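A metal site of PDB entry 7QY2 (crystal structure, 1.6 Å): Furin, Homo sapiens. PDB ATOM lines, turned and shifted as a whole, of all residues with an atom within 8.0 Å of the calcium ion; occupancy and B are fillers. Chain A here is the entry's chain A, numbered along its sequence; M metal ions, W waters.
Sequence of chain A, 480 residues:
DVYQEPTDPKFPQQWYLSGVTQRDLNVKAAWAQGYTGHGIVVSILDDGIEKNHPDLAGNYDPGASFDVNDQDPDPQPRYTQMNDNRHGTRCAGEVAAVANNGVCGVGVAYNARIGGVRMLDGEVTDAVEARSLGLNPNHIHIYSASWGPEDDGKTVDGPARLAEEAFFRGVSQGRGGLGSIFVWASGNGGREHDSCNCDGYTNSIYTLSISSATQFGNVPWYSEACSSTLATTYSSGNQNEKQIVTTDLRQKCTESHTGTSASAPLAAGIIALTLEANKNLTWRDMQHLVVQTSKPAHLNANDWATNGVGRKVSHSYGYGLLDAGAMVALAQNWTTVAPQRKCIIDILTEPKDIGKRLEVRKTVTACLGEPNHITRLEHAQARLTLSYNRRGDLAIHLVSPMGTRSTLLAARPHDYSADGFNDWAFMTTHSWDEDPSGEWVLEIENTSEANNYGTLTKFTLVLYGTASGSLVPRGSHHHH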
ATOM      1  N   LYS A  51      19.549   4.366 -22.741  1.00  0.00           N
ATOM      2  CA  LYS A  51      18.353   3.805 -23.334  1.00  0.00           C
ATOM      3  C   LYS A  51      18.107   4.345 -24.739  1.00  0.00           C
ATOM      4  O   LYS A  51      17.390   3.697 -25.510  1.00  0.00           O
ATOM      5  CB  LYS A  51      17.137   4.061 -22.434  1.00  0.00           C
ATOM      6  CG  LYS A  51      16.736   5.514 -22.264  1.00  0.00           C
ATOM      7  CD  LYS A  51      15.716   5.636 -21.140  1.00  0.00           C
ATOM      8  CE  LYS A  51      15.358   7.089 -20.881  1.00  0.00           C
ATOM      9  NZ  LYS A  51      16.536   7.832 -20.372  1.00  0.00           N
ATOM     10  N   PHE A  66      15.263   0.753 -13.593  1.00  0.00           N
ATOM     11  CA  PHE A  66      15.083   1.673 -12.478  1.00  0.00           C
ATOM     12  C   PHE A  66      16.420   2.282 -12.098  1.00  0.00           C
ATOM     13  O   PHE A  66      17.489   1.790 -12.493  1.00  0.00           O
ATOM     14  CB  PHE A  66      14.467   0.963 -11.262  1.00  0.00           C
ATOM     15  CG  PHE A  66      13.665   1.874 -10.386  1.00  0.00           C
ATOM     16  CD1 PHE A  66      12.358   2.201 -10.718  1.00  0.00           C
ATOM     17  CD2 PHE A  66      14.196   2.401  -9.226  1.00  0.00           C
ATOM     18  CE1 PHE A  66      11.616   3.042  -9.922  1.00  0.00           C
ATOM     19  CE2 PHE A  66      13.455   3.242  -8.416  1.00  0.00           C
ATOM     20  CZ  PHE A  66      12.162   3.556  -8.772  1.00  0.00           C
ATOM     21  N   ASP A  67      16.363   3.372 -11.342  1.00  0.00           N
ATOM     22  CA  ASP A  67      17.535   4.080 -10.856  1.00  0.00           C
ATOM     23  C   ASP A  67      17.452   4.089  -9.335  1.00  0.00           C
ATOM     24  O   ASP A  67      16.792   4.941  -8.736  1.00  0.00           O
ATOM     25  CB  ASP A  67      17.587   5.496 -11.413  1.00  0.00           C
ATOM     26  CG  ASP A  67      18.820   6.257 -10.986  1.00  0.00           C
ATOM     27  OD1 ASP A  67      19.553   5.779 -10.089  1.00  0.00           O
ATOM     28  OD2 ASP A  67      19.060   7.351 -11.546  1.00  0.00           O
ATOM     29  N   VAL A  68      18.128   3.122  -8.713  1.00  0.00           N
ATOM     30  CA  VAL A  68      18.122   3.024  -7.262  1.00  0.00           C
ATOM     31  C   VAL A  68      19.104   3.986  -6.622  1.00  0.00           C
ATOM     32  O   VAL A  68      18.948   4.313  -5.433  1.00  0.00           O
ATOM     33  CB  VAL A  68      18.407   1.567  -6.868  1.00  0.00           C
ATOM     34  CG1 VAL A  68      18.427   1.416  -5.374  1.00  0.00           C
ATOM     35  CG2 VAL A  68      17.372   0.627  -7.488  1.00  0.00           C
ATOM     36  N   ASN A  69      20.086   4.491  -7.375  1.00  0.00           N
ATOM     37  CA  ASN A  69      21.064   5.413  -6.810  1.00  0.00           C
ATOM     38  C   ASN A  69      20.439   6.782  -6.551  1.00  0.00           C
ATOM     39  O   ASN A  69      20.694   7.414  -5.526  1.00  0.00           O
ATOM     40  CB  ASN A  69      22.279   5.559  -7.722  1.00  0.00           C
ATOM     41  CG  ASN A  69      23.130   4.291  -7.812  1.00  0.00           C
ATOM     42  OD1 ASN A  69      23.547   3.885  -8.905  1.00  0.00           O
ATOM     43  ND2 ASN A  69      23.426   3.679  -6.672  1.00  0.00           N
ATOM     44  N   ASP A  70      19.626   7.266  -7.499  1.00  0.00           N
ATOM     45  CA  ASP A  70      18.951   8.556  -7.385  1.00  0.00           C
ATOM     46  C   ASP A  70      17.453   8.423  -7.119  1.00  0.00           C
ATOM     47  O   ASP A  70      16.768   9.438  -6.997  1.00  0.00           O
ATOM     48  CB  ASP A  70      19.146   9.376  -8.674  1.00  0.00           C
ATOM     49  CG  ASP A  70      20.488  10.079  -8.728  1.00  0.00           C
ATOM     50  OD1 ASP A  70      21.112  10.292  -7.670  1.00  0.00           O
ATOM     51  OD2 ASP A  70      20.928  10.437  -9.850  1.00  0.00           O
ATOM     52  N   GLN A  71      16.927   7.198  -7.045  1.00  0.00           N
ATOM     53  CA  GLN A  71      15.536   6.937  -6.697  1.00  0.00           C
ATOM     54  C   GLN A  71      14.581   7.563  -7.708  1.00  0.00           C
ATOM     55  O   GLN A  71      13.770   8.440  -7.388  1.00  0.00           O
ATOM     56  CB  GLN A  71      15.249   7.434  -5.272  1.00  0.00           C
ATOM     57  CG  GLN A  71      16.207   6.859  -4.236  1.00  0.00           C
ATOM     58  CD  GLN A  71      15.624   6.854  -2.827  1.00  0.00           C
ATOM     59  N   ASP A  72      14.675   7.081  -8.947  1.00  0.00           N
ATOM     60  CA  ASP A  72      13.759   7.484 -10.014  1.00  0.00           C
ATOM     61  C   ASP A  72      13.705   6.353 -11.028  1.00  0.00           C
ATOM     62  O   ASP A  72      14.468   5.386 -10.924  1.00  0.00           O
ATOM     63  CB  ASP A  72      14.188   8.808 -10.670  1.00  0.00           C
ATOM     64  CG  ASP A  72      15.533   8.727 -11.389  1.00  0.00           C
ATOM     65  OD1 ASP A  72      15.634   7.975 -12.386  1.00  0.00           O
ATOM     66  OD2 ASP A  72      16.468   9.442 -10.992  1.00  0.00           O
ATOM     67  N   PRO A  73      12.795   6.417 -12.000  1.00  0.00           N
ATOM     68  CA  PRO A  73      12.641   5.288 -12.928  1.00  0.00           C
ATOM     69  C   PRO A  73      13.662   5.243 -14.046  1.00  0.00           C
ATOM     70  O   PRO A  73      13.706   4.242 -14.773  1.00  0.00           O
ATOM     71  CB  PRO A  73      11.231   5.493 -13.510  1.00  0.00           C
ATOM     72  CG  PRO A  73      10.609   6.624 -12.773  1.00  0.00           C
ATOM     73  CD  PRO A  73      11.723   7.422 -12.170  1.00  0.00           C
ATOM     74  N   ASP A  74      14.465   6.296 -14.204  1.00  0.00           N
ATOM     75  CA  ASP A  74      15.225   6.509 -15.425  1.00  0.00           C
ATOM     76  C   ASP A  74      16.678   6.115 -15.202  1.00  0.00           C
ATOM     77  O   ASP A  74      17.391   6.813 -14.470  1.00  0.00           O
ATOM     78  CB  ASP A  74      15.123   7.987 -15.838  1.00  0.00           C
ATOM     79  CG  ASP A  74      15.882   8.310 -17.108  1.00  0.00           C
ATOM     80  OD1 ASP A  74      16.583   7.438 -17.654  1.00  0.00           O
ATOM     81  OD2 ASP A  74      15.765   9.464 -17.566  1.00  0.00           O
ATOM     82  N   PRO A  75      17.159   5.033 -15.819  1.00  0.00           N
ATOM     83  CA  PRO A  75      18.514   4.547 -15.531  1.00  0.00           C
ATOM     84  C   PRO A  75      19.603   5.150 -16.399  1.00  0.00           C
ATOM     85  O   PRO A  75      20.699   4.571 -16.504  1.00  0.00           O
ATOM     86  CB  PRO A  75      18.398   3.040 -15.801  1.00  0.00           C
ATOM     87  CG  PRO A  75      17.485   3.040 -17.048  1.00  0.00           C
ATOM     88  CD  PRO A  75      16.439   4.105 -16.717  1.00  0.00           C
ATOM     89  N   GLN A  76      19.327   6.266 -17.054  1.00  0.00           N
ATOM     90  CA  GLN A  76      20.328   6.868 -17.922  1.00  0.00           C
ATOM     91  C   GLN A  76      21.633   7.057 -17.159  1.00  0.00           C
ATOM     92  O   GLN A  76      21.613   7.503 -16.007  1.00  0.00           O
ATOM     93  CB  GLN A  76      19.825   8.210 -18.450  1.00  0.00           C
ATOM     94  CG  GLN A  76      20.623   8.753 -19.642  1.00  0.00           C
ATOM     95  CD  GLN A  76      20.278   8.057 -20.942  1.00  0.00           C
ATOM     96  OE1 GLN A  76      19.288   7.345 -21.043  1.00  0.00           O
ATOM     97  NE2 GLN A  76      21.113   8.267 -21.963  1.00  0.00           N
ATOM     98  N   PRO A  77      22.781   6.748 -17.767  1.00  0.00           N
ATOM     99  CA  PRO A  77      24.047   6.909 -17.046  1.00  0.00           C
ATOM    100  C   PRO A  77      24.421   8.358 -16.793  1.00  0.00           C
ATOM    101  O   PRO A  77      23.978   9.279 -17.500  1.00  0.00           O
ATOM    102  CB  PRO A  77      25.073   6.251 -17.984  1.00  0.00           C
ATOM    103  CG  PRO A  77      24.273   5.408 -18.942  1.00  0.00           C
ATOM    104  CD  PRO A  77      22.943   6.084 -19.067  1.00  0.00           C
ATOM    105  N   ARG A  78      25.254   8.558 -15.781  1.00  0.00           N
ATOM    106  CA  ARG A  78      25.889   9.852 -15.523  1.00  0.00           C
ATOM    107  C   ARG A  78      27.103   9.999 -16.435  1.00  0.00           C
ATOM    108  O   ARG A  78      28.051   9.206 -16.339  1.00  0.00           O
ATOM    109  CB  ARG A  78      26.290   9.928 -14.047  1.00  0.00           C
ATOM    110  CG  ARG A  78      26.930  11.235 -13.597  1.00  0.00           C
ATOM    111  CD  ARG A  78      27.162  11.215 -12.087  1.00  0.00           C
ATOM    112  NE  ARG A  78      27.995  10.067 -11.718  1.00  0.00           N
ATOM    113  CZ  ARG A  78      29.306  10.117 -11.557  1.00  0.00           C
ATOM    114  NH1 ARG A  78      29.955  11.268 -11.709  1.00  0.00           N
ATOM    115  NH2 ARG A  78      29.983   9.023 -11.229  1.00  0.00           N
ATOM    116  N   ARG A 118      20.259   1.201 -12.583  1.00  0.00           N
ATOM    117  CA  ARG A 118      21.365   2.057 -12.188  1.00  0.00           C
ATOM    118  C   ARG A 118      21.519   1.908 -10.675  1.00  0.00           C
ATOM    119  O   ARG A 118      20.746   2.486  -9.911  1.00  0.00           O
ATOM    120  CB  ARG A 118      21.091   3.495 -12.612  1.00  0.00           C
ATOM    121  CG  ARG A 118      22.215   4.464 -12.302  1.00  0.00           C
ATOM    122  CD  ARG A 118      22.011   5.865 -12.934  1.00  0.00           C
ATOM    123  NE  ARG A 118      23.112   6.707 -12.525  1.00  0.00           N
ATOM    124  CZ  ARG A 118      23.024   7.689 -11.626  1.00  0.00           C
ATOM    125  NH1 ARG A 118      21.871   7.994 -11.054  1.00  0.00           N
ATOM    126  NH2 ARG A 118      24.118   8.384 -11.299  1.00  0.00           N
HETATM  127 CA    CA M   1      17.908   8.685 -12.972  1.00  0.00          CA
HETATM  128  O   HOH W   1      16.909  10.533 -14.242  1.00  0.00           O
HETATM  129  O   HOH W   2      19.587   8.890 -14.583  1.00  0.00           O
HETATM  130  O   HOH W   3      19.306  10.480 -12.036  1.00  0.00           O
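N of Asp 70 is in hydrogen-bond range of OD1 of Asp 67 (3.0 Å). The backbone NH (N) of Gln 76 lies within hydrogen-bond range of the side-chain carboxylate (OD1) of Asp 74 (3.0 Å). N of Asn 69 is in hydrogen-bond range of OD1 of Asp 67, 3.1 Å away. The side-chain carboxylate of Asp 74 is in salt-bridge range of the side-chain amino group of Lys 51, 2.7 Å away. OD1 of Asp 67 lies within salt-bridge range of NH1 of Arg 118 (3.3 Å).
Of the 15 residues printed, 3 come within 4 Å of the calcium ion. Along chain A the residues within 4 Å of the calcium ion span positions 67 to 74.
OD2 of Asp 67 binds the calcium ion (2.3 Å). Water W2 is bound to the calcium ion (2.3 Å). OD1 of Asp 72 binds the calcium ion (2.5 Å). O of Asp 74 is bound to the calcium ion, 2.5 Å away. Water W1 is bound to the calcium ion. Water W3 is bound to the calcium ion, 2.5 Å away. The calcium ion is bound by OD2 of Asp 72, at 2.6 Å.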
